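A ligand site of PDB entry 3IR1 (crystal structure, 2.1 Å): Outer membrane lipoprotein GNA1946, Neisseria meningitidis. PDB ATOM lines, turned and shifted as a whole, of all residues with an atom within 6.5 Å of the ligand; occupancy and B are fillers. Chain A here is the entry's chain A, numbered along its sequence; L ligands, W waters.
Water W2 lies within hydrogen-bond range of O1 of the ligand (2.5 Å), O of Ala 82 (3.3 Å) and NH1 of Arg 114 (3.3 Å). Water W3 lies within hydrogen-bond range of O2 of the ligand, N of Gly 172, N of Leu 84 and O of Ala 82. Water W1 lies within hydrogen-bond range of the backbone carbonyl oxygen (O) of Phe 56 (2.7 Å), a nitrogen (N1) of the ligand (2.9 Å), the side-chain hydroxyl (OG1) of Thr 8 (2.9 Å) and the side-chain amide oxygen (OD1) of Asn 173 (3.4 Å). Water W4 lies within hydrogen-bond range of O of Ala 82 (2.8 Å), N1 of the ligand (3.0 Å) and N of Asn 173 (3.0 Å).
Residues that only touch the ligand: Phe 12 (3.7 Å), Tyr 39 (3.5 Å), Phe 56 (3.1 Å), Gln 57 (3.7 Å), Tyr 61 (3.6 Å), Thr 81 (3.6 Å), Asn 173 (3.5 Å) and Tyr 194 (3.98 Å). Within 4 Å of the ligand: Phe 12, Tyr 39, Phe 56, Gln 57, His 58, Tyr 61, Thr 81, Asn 111, Arg 114, Asn 171, Asn 173, Tyr 194 and Asn 196. Along chain A the residues within 4 Å of the ligand span positions 12 to 196.
The guanidinium group of Arg 114 sits close to the side-chain amide nitrogen of Asn 171, at 3.4 Å. NH2 of Arg 114 lies within hydrogen-bond range of OD1 of Asn 111, 3.0 Å away. The side-chain amide oxygen (OD1) of Asn 196 lies close to the backbone carbonyl oxygen (O) of Phe 56 (3.3 Å). N of Asn 196 lies within hydrogen-bond range of OG1 of Thr 81 (2.8 Å). The backbone carbonyl oxygen of Tyr 194 lies within hydrogen-bond range of the side-chain amide nitrogen of Asn 196 (2.9 Å). ND2 of Asn 171 lies within hydrogen-bond range of OD1 of Asn 111 (3.0 Å). The side-chain amide oxygen (OD1) of Asn 111 sits at hydrogen-bond distance from a ring nitrogen (NE2) of His 58 (3.1 Å). OD2 of Asp 108 lies within hydrogen-bond range of ND2 of Asn 111 (2.6 Å).
NH2 of Arg 114 lies within salt-bridge range of O2 of the ligand, 2.5 Å away. The side-chain amide oxygen (OD1) of Asn 196 lies within hydrogen-bond range of a nitrogen (N1) of the ligand (2.7 Å). O2 of the ligand is in hydrogen-bond range of ND2 of Asn 171 (2.9 Å). S1 of the ligand lies close to NE2 of His 58. The side-chain amide nitrogen (ND2) of Asn 111 lies close to a sulfur (S1) of the ligand (3.6 Å).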
ATOM      1  N   THR A   8      15.874  25.826  -9.765  1.00  0.00           N
ATOM      2  CA  THR A   8      14.670  25.254  -9.180  1.00  0.00           C
ATOM      3  C   THR A   8      13.629  26.250  -9.662  1.00  0.00           C
ATOM      4  O   THR A   8      13.931  27.411  -9.935  1.00  0.00           O
ATOM      5  CB  THR A   8      14.674  25.257  -7.622  1.00  0.00           C
ATOM      6  OG1 THR A   8      15.399  26.391  -7.128  1.00  0.00           O
ATOM      7  CG2 THR A   8      15.270  23.951  -7.082  1.00  0.00           C
ATOM      8  N   ASP A  11      11.675  31.668  -7.738  1.00  0.00           N
ATOM      9  CA  ASP A  11      12.595  32.791  -7.665  1.00  0.00           C
ATOM     10  C   ASP A  11      13.890  32.733  -8.475  1.00  0.00           C
ATOM     11  O   ASP A  11      14.175  33.673  -9.224  1.00  0.00           O
ATOM     12  CB  ASP A  11      12.883  33.181  -6.200  1.00  0.00           C
ATOM     13  CG  ASP A  11      13.436  32.034  -5.361  1.00  0.00           C
ATOM     14  OD1 ASP A  11      13.444  32.209  -4.124  1.00  0.00           O
ATOM     15  OD2 ASP A  11      13.874  30.991  -5.884  1.00  0.00           O
ATOM     16  N   PHE A  12      14.668  31.671  -8.371  1.00  0.00           N
ATOM     17  CA  PHE A  12      15.909  31.617  -9.145  1.00  0.00           C
ATOM     18  C   PHE A  12      15.614  31.600 -10.635  1.00  0.00           C
ATOM     19  O   PHE A  12      16.370  32.163 -11.428  1.00  0.00           O
ATOM     20  CB  PHE A  12      16.751  30.410  -8.723  1.00  0.00           C
ATOM     21  CG  PHE A  12      17.271  30.498  -7.316  1.00  0.00           C
ATOM     22  CD1 PHE A  12      17.816  31.698  -6.829  1.00  0.00           C
ATOM     23  CD2 PHE A  12      17.256  29.391  -6.476  1.00  0.00           C
ATOM     24  CE1 PHE A  12      18.335  31.776  -5.534  1.00  0.00           C
ATOM     25  CE2 PHE A  12      17.771  29.462  -5.171  1.00  0.00           C
ATOM     26  CZ  PHE A  12      18.312  30.658  -4.705  1.00  0.00           C
ATOM     27  N   TYR A  39      15.650  18.903  -5.846  1.00  0.00           N
ATOM     28  CA  TYR A  39      17.041  19.278  -5.589  1.00  0.00           C
ATOM     29  C   TYR A  39      18.071  18.313  -6.185  1.00  0.00           C
ATOM     30  O   TYR A  39      19.237  18.661  -6.347  1.00  0.00           O
ATOM     31  CB  TYR A  39      17.310  19.360  -4.084  1.00  0.00           C
ATOM     32  CG  TYR A  39      16.620  20.487  -3.344  1.00  0.00           C
ATOM     33  CD1 TYR A  39      16.250  21.661  -4.001  1.00  0.00           C
ATOM     34  CD2 TYR A  39      16.450  20.417  -1.961  1.00  0.00           C
ATOM     35  CE1 TYR A  39      15.737  22.756  -3.277  1.00  0.00           C
ATOM     36  CE2 TYR A  39      15.945  21.495  -1.245  1.00  0.00           C
ATOM     37  CZ  TYR A  39      15.591  22.664  -1.899  1.00  0.00           C
ATOM     38  OH  TYR A  39      15.140  23.726  -1.165  1.00  0.00           O
ATOM     39  N   PHE A  56      20.552  26.845  -7.609  1.00  0.00           N
ATOM     40  CA  PHE A  56      19.480  26.321  -6.759  1.00  0.00           C
ATOM     41  C   PHE A  56      19.956  25.799  -5.402  1.00  0.00           C
ATOM     42  O   PHE A  56      19.133  25.478  -4.548  1.00  0.00           O
ATOM     43  CB  PHE A  56      18.801  25.152  -7.470  1.00  0.00           C
ATOM     44  CG  PHE A  56      19.584  23.854  -7.377  1.00  0.00           C
ATOM     45  CD1 PHE A  56      19.199  22.846  -6.488  1.00  0.00           C
ATOM     46  CD2 PHE A  56      20.730  23.649  -8.143  1.00  0.00           C
ATOM     47  CE1 PHE A  56      19.938  21.668  -6.360  1.00  0.00           C
ATOM     48  CE2 PHE A  56      21.477  22.469  -8.030  1.00  0.00           C
ATOM     49  CZ  PHE A  56      21.083  21.478  -7.134  1.00  0.00           C
ATOM     50  N   GLN A  57      21.268  25.729  -5.197  1.00  0.00           N
ATOM     51  CA  GLN A  57      21.800  25.145  -3.957  1.00  0.00           C
ATOM     52  C   GLN A  57      22.824  25.978  -3.203  1.00  0.00           C
ATOM     53  O   GLN A  57      23.365  26.949  -3.723  1.00  0.00           O
ATOM     54  CB  GLN A  57      22.464  23.815  -4.308  1.00  0.00           C
ATOM     55  CG  GLN A  57      23.856  24.000  -4.950  1.00  0.00           C
ATOM     56  CD  GLN A  57      24.284  22.834  -5.830  1.00  0.00           C
ATOM     57  OE1 GLN A  57      24.349  21.679  -5.382  1.00  0.00           O
ATOM     58  NE2 GLN A  57      24.591  23.127  -7.089  1.00  0.00           N
ATOM     59  N   HIS A  58      23.096  25.562  -1.967  1.00  0.00           N
ATOM     60  CA  HIS A  58      24.122  26.227  -1.163  1.00  0.00           C
ATOM     61  C   HIS A  58      25.370  25.331  -1.227  1.00  0.00           C
ATOM     62  O   HIS A  58      25.293  24.182  -1.684  1.00  0.00           O
ATOM     63  CB  HIS A  58      23.653  26.469   0.285  1.00  0.00           C
ATOM     64  CG  HIS A  58      22.929  25.316   0.911  1.00  0.00           C
ATOM     65  ND1 HIS A  58      23.554  24.129   1.220  1.00  0.00           N
ATOM     66  CD2 HIS A  58      21.651  25.202   1.341  1.00  0.00           C
ATOM     67  CE1 HIS A  58      22.693  23.327   1.828  1.00  0.00           C
ATOM     68  NE2 HIS A  58      21.531  23.952   1.916  1.00  0.00           N
ATOM     69  N   TYR A  61      25.415  21.681   0.377  1.00  0.00           N
ATOM     70  CA  TYR A  61      24.665  20.692  -0.385  1.00  0.00           C
ATOM     71  C   TYR A  61      25.499  20.280  -1.597  1.00  0.00           C
ATOM     72  O   TYR A  61      25.664  19.092  -1.900  1.00  0.00           O
ATOM     73  CB  TYR A  61      23.312  21.262  -0.828  1.00  0.00           C
ATOM     74  CG  TYR A  61      22.455  20.272  -1.577  1.00  0.00           C
ATOM     75  CD1 TYR A  61      22.636  20.052  -2.952  1.00  0.00           C
ATOM     76  CD2 TYR A  61      21.478  19.525  -0.907  1.00  0.00           C
ATOM     77  CE1 TYR A  61      21.875  19.110  -3.643  1.00  0.00           C
ATOM     78  CE2 TYR A  61      20.713  18.570  -1.600  1.00  0.00           C
ATOM     79  CZ  TYR A  61      20.921  18.370  -2.959  1.00  0.00           C
ATOM     80  OH  TYR A  61      20.184  17.429  -3.650  1.00  0.00           O
ATOM     81  N   LEU A  62      26.043  21.267  -2.281  1.00  0.00           N
ATOM     82  CA  LEU A  62      26.888  21.046  -3.444  1.00  0.00           C
ATOM     83  C   LEU A  62      28.033  20.106  -3.072  1.00  0.00           C
ATOM     84  O   LEU A  62      28.278  19.112  -3.767  1.00  0.00           O
ATOM     85  CB  LEU A  62      27.490  22.378  -3.909  1.00  0.00           C
ATOM     86  CG  LEU A  62      27.897  22.614  -5.380  1.00  0.00           C
ATOM     87  CD1 LEU A  62      29.142  23.438  -5.371  1.00  0.00           C
ATOM     88  CD2 LEU A  62      28.128  21.335  -6.133  1.00  0.00           C
ATOM     89  N   THR A  81      19.380  34.991  -1.866  1.00  0.00           N
ATOM     90  CA  THR A  81      18.736  33.757  -1.450  1.00  0.00           C
ATOM     91  C   THR A  81      17.606  33.886  -0.417  1.00  0.00           C
ATOM     92  O   THR A  81      17.723  34.634   0.544  1.00  0.00           O
ATOM     93  CB  THR A  81      19.804  32.790  -0.894  1.00  0.00           C
ATOM     94  OG1 THR A  81      20.809  32.560  -1.905  1.00  0.00           O
ATOM     95  CG2 THR A  81      19.178  31.460  -0.462  1.00  0.00           C
ATOM     96  N   ALA A  82      16.523  33.140  -0.625  1.00  0.00           N
ATOM     97  CA  ALA A  82      15.397  33.161   0.304  1.00  0.00           C
ATOM     98  C   ALA A  82      15.890  32.384   1.519  1.00  0.00           C
ATOM     99  O   ALA A  82      16.205  31.207   1.420  1.00  0.00           O
ATOM    100  CB  ALA A  82      14.180  32.479  -0.310  1.00  0.00           C
ATOM    101  N   PRO A  83      15.943  33.039   2.688  1.00  0.00           N
ATOM    102  CA  PRO A  83      16.407  32.414   3.939  1.00  0.00           C
ATOM    103  C   PRO A  83      15.558  31.274   4.499  1.00  0.00           C
ATOM    104  O   PRO A  83      14.352  31.207   4.263  1.00  0.00           O
ATOM    105  CB  PRO A  83      16.479  33.602   4.896  1.00  0.00           C
ATOM    106  CG  PRO A  83      15.313  34.440   4.432  1.00  0.00           C
ATOM    107  CD  PRO A  83      15.485  34.419   2.928  1.00  0.00           C
ATOM    108  N   LEU A  84      16.207  30.390   5.244  1.00  0.00           N
ATOM    109  CA  LEU A  84      15.507  29.269   5.855  1.00  0.00           C
ATOM    110  C   LEU A  84      14.724  29.808   7.061  1.00  0.00           C
ATOM    111  O   LEU A  84      15.216  30.673   7.797  1.00  0.00           O
ATOM    112  CB  LEU A  84      16.497  28.215   6.324  1.00  0.00           C
ATOM    113  CG  LEU A  84      15.853  27.022   7.051  1.00  0.00           C
ATOM    114  CD1 LEU A  84      15.036  26.201   6.055  1.00  0.00           C
ATOM    115  CD2 LEU A  84      16.925  26.164   7.696  1.00  0.00           C
ATOM    116  N   ASP A 108      17.064  15.673   3.693  1.00  0.00           N
ATOM    117  CA  ASP A 108      18.409  15.464   3.140  1.00  0.00           C
ATOM    118  C   ASP A 108      19.377  16.008   4.198  1.00  0.00           C
ATOM    119  O   ASP A 108      19.113  17.028   4.840  1.00  0.00           O
ATOM    120  CB  ASP A 108      18.582  16.186   1.800  1.00  0.00           C
ATOM    121  CG  ASP A 108      18.346  17.673   1.901  1.00  0.00           C
ATOM    122  OD1 ASP A 108      17.174  18.062   2.096  1.00  0.00           O
ATOM    123  OD2 ASP A 108      19.327  18.436   1.789  1.00  0.00           O
ATOM    124  N   SER A 110      22.477  17.803   4.441  1.00  0.00           N
ATOM    125  CA  SER A 110      22.970  19.181   4.556  1.00  0.00           C
ATOM    126  C   SER A 110      21.885  20.149   5.054  1.00  0.00           C
ATOM    127  O   SER A 110      22.172  21.060   5.823  1.00  0.00           O
ATOM    128  CB  SER A 110      23.568  19.679   3.238  1.00  0.00           C
ATOM    129  OG  SER A 110      22.588  19.870   2.238  1.00  0.00           O
ATOM    130  N   ASN A 111      20.654  19.939   4.619  1.00  0.00           N
ATOM    131  CA  ASN A 111      19.565  20.812   5.054  1.00  0.00           C
ATOM    132  C   ASN A 111      19.016  20.428   6.420  1.00  0.00           C
ATOM    133  O   ASN A 111      18.621  21.293   7.196  1.00  0.00           O
ATOM    134  CB  ASN A 111      18.454  20.823   4.003  1.00  0.00           C
ATOM    135  CG  ASN A 111      18.809  21.670   2.813  1.00  0.00           C
ATOM    136  OD1 ASN A 111      18.840  22.899   2.907  1.00  0.00           O
ATOM    137  ND2 ASN A 111      19.123  21.025   1.698  1.00  0.00           N
ATOM    138  N   ARG A 114      20.802  22.041   9.297  1.00  0.00           N
ATOM    139  CA  ARG A 114      20.365  23.414   9.549  1.00  0.00           C
ATOM    140  C   ARG A 114      19.200  23.499  10.531  1.00  0.00           C
ATOM    141  O   ARG A 114      19.114  24.456  11.305  1.00  0.00           O
ATOM    142  CB  ARG A 114      19.946  24.083   8.255  1.00  0.00           C
ATOM    143  CG  ARG A 114      21.035  24.186   7.226  1.00  0.00           C
ATOM    144  CD  ARG A 114      20.813  25.437   6.410  1.00  0.00           C
ATOM    145  NE  ARG A 114      19.976  25.197   5.263  1.00  0.00           N
ATOM    146  CZ  ARG A 114      19.444  26.160   4.507  1.00  0.00           C
ATOM    147  NH1 ARG A 114      19.661  27.435   4.797  1.00  0.00           N
ATOM    148  NH2 ARG A 114      18.733  25.824   3.450  1.00  0.00           N
ATOM    149  N   VAL A 170      10.874  25.404   6.674  1.00  0.00           N
ATOM    150  CA  VAL A 170      10.801  25.345   5.212  1.00  0.00           C
ATOM    151  C   VAL A 170      11.903  26.082   4.440  1.00  0.00           C
ATOM    152  O   VAL A 170      12.249  27.220   4.778  1.00  0.00           O
ATOM    153  CB  VAL A 170       9.419  25.938   4.765  1.00  0.00           C
ATOM    154  CG1 VAL A 170       9.186  25.719   3.282  1.00  0.00           C
ATOM    155  CG2 VAL A 170       8.308  25.315   5.599  1.00  0.00           C
ATOM    156  N   ASN A 171      12.439  25.432   3.406  1.00  0.00           N
ATOM    157  CA  ASN A 171      13.473  26.040   2.569  1.00  0.00           C
ATOM    158  C   ASN A 171      12.777  27.214   1.853  1.00  0.00           C
ATOM    159  O   ASN A 171      11.617  27.093   1.440  1.00  0.00           O
ATOM    160  CB  ASN A 171      14.028  25.070   1.510  1.00  0.00           C
ATOM    161  CG  ASN A 171      14.796  23.903   2.107  1.00  0.00           C
ATOM    162  OD1 ASN A 171      14.229  22.857   2.409  1.00  0.00           O
ATOM    163  ND2 ASN A 171      16.108  24.086   2.290  1.00  0.00           N
ATOM    164  N   GLY A 172      13.490  28.329   1.703  1.00  0.00           N
ATOM    165  CA  GLY A 172      12.918  29.497   1.065  1.00  0.00           C
ATOM    166  C   GLY A 172      12.321  29.369  -0.317  1.00  0.00           C
ATOM    167  O   GLY A 172      11.243  29.903  -0.575  1.00  0.00           O
ATOM    168  N   ASN A 173      13.006  28.680  -1.225  1.00  0.00           N
ATOM    169  CA  ASN A 173      12.494  28.541  -2.592  1.00  0.00           C
ATOM    170  C   ASN A 173      11.118  27.875  -2.565  1.00  0.00           C
ATOM    171  O   ASN A 173      10.226  28.267  -3.314  1.00  0.00           O
ATOM    172  CB  ASN A 173      13.458  27.742  -3.468  1.00  0.00           C
ATOM    173  CG  ASN A 173      13.603  26.292  -3.030  1.00  0.00           C
ATOM    174  OD1 ASN A 173      14.213  25.996  -2.015  1.00  0.00           O
ATOM    175  ND2 ASN A 173      13.035  25.387  -3.820  1.00  0.00           N
ATOM    176  N   TYR A 194      24.721  29.566   4.107  1.00  0.00           N
ATOM    177  CA  TYR A 194      23.860  28.880   3.137  1.00  0.00           C
ATOM    178  C   TYR A 194      23.307  29.726   1.997  1.00  0.00           C
ATOM    179  O   TYR A 194      22.363  29.328   1.317  1.00  0.00           O
ATOM    180  CB  TYR A 194      22.711  28.203   3.887  1.00  0.00           C
ATOM    181  CG  TYR A 194      23.208  27.134   4.835  1.00  0.00           C
ATOM    182  CD1 TYR A 194      23.501  25.852   4.377  1.00  0.00           C
ATOM    183  CD2 TYR A 194      23.431  27.422   6.182  1.00  0.00           C
ATOM    184  CE1 TYR A 194      23.989  24.875   5.249  1.00  0.00           C
ATOM    185  CE2 TYR A 194      23.923  26.458   7.055  1.00  0.00           C
ATOM    186  CZ  TYR A 194      24.204  25.188   6.583  1.00  0.00           C
ATOM    187  OH  TYR A 194      24.672  24.218   7.443  1.00  0.00           O
ATOM    188  N   VAL A 195      23.889  30.904   1.795  1.00  0.00           N
ATOM    189  CA  VAL A 195      23.470  31.752   0.697  1.00  0.00           C
ATOM    190  C   VAL A 195      23.843  30.900  -0.512  1.00  0.00           C
ATOM    191  O   VAL A 195      24.950  30.348  -0.582  1.00  0.00           O
ATOM    192  CB  VAL A 195      24.240  33.071   0.701  1.00  0.00           C
ATOM    193  CG1 VAL A 195      23.840  33.939  -0.501  1.00  0.00           C
ATOM    194  CG2 VAL A 195      23.966  33.797   2.006  1.00  0.00           C
ATOM    195  N   ASN A 196      22.912  30.761  -1.451  1.00  0.00           N
ATOM    196  CA  ASN A 196      23.137  29.910  -2.618  1.00  0.00           C
ATOM    197  C   ASN A 196      24.197  30.356  -3.603  1.00  0.00           C
ATOM    198  O   ASN A 196      24.496  31.547  -3.735  1.00  0.00           O
ATOM    199  CB  ASN A 196      21.803  29.686  -3.357  1.00  0.00           C
ATOM    200  CG  ASN A 196      20.828  28.844  -2.553  1.00  0.00           C
ATOM    201  OD1 ASN A 196      19.813  28.377  -3.084  1.00  0.00           O
ATOM    202  ND2 ASN A 196      21.140  28.634  -1.267  1.00  0.00           N
HETATM  203  N1  LIG L   1      17.455  27.385  -2.080  1.00  0.00           N
HETATM  204  C1  LIG L   1      17.594  26.318  -1.042  1.00  0.00           C
HETATM  205  C2  LIG L   1      17.974  26.968   0.307  1.00  0.00           C
HETATM  206  O1  LIG L   1      18.780  27.924   0.292  1.00  0.00           O
HETATM  207  C3  LIG L   1      18.678  25.329  -1.467  1.00  0.00           C
HETATM  208  C4  LIG L   1      18.791  24.086  -0.580  1.00  0.00           C
HETATM  209  S1  LIG L   1      20.215  23.049  -1.041  1.00  0.00           S
HETATM  210  C5  LIG L   1      19.555  22.293  -2.537  1.00  0.00           C
HETATM  211  O2  LIG L   1      17.459  26.504   1.351  1.00  0.00           O
HETATM  212  O   HOH W   1      16.574  26.181  -4.514  1.00  0.00           O
HETATM  213  O   HOH W   2      18.756  29.377   2.329  1.00  0.00           O
HETATM  214  O   HOH W   3      16.204  28.219   2.880  1.00  0.00           O
HETATM  215  O   HOH W   4      15.875  29.556  -0.808  1.00  0.00           O
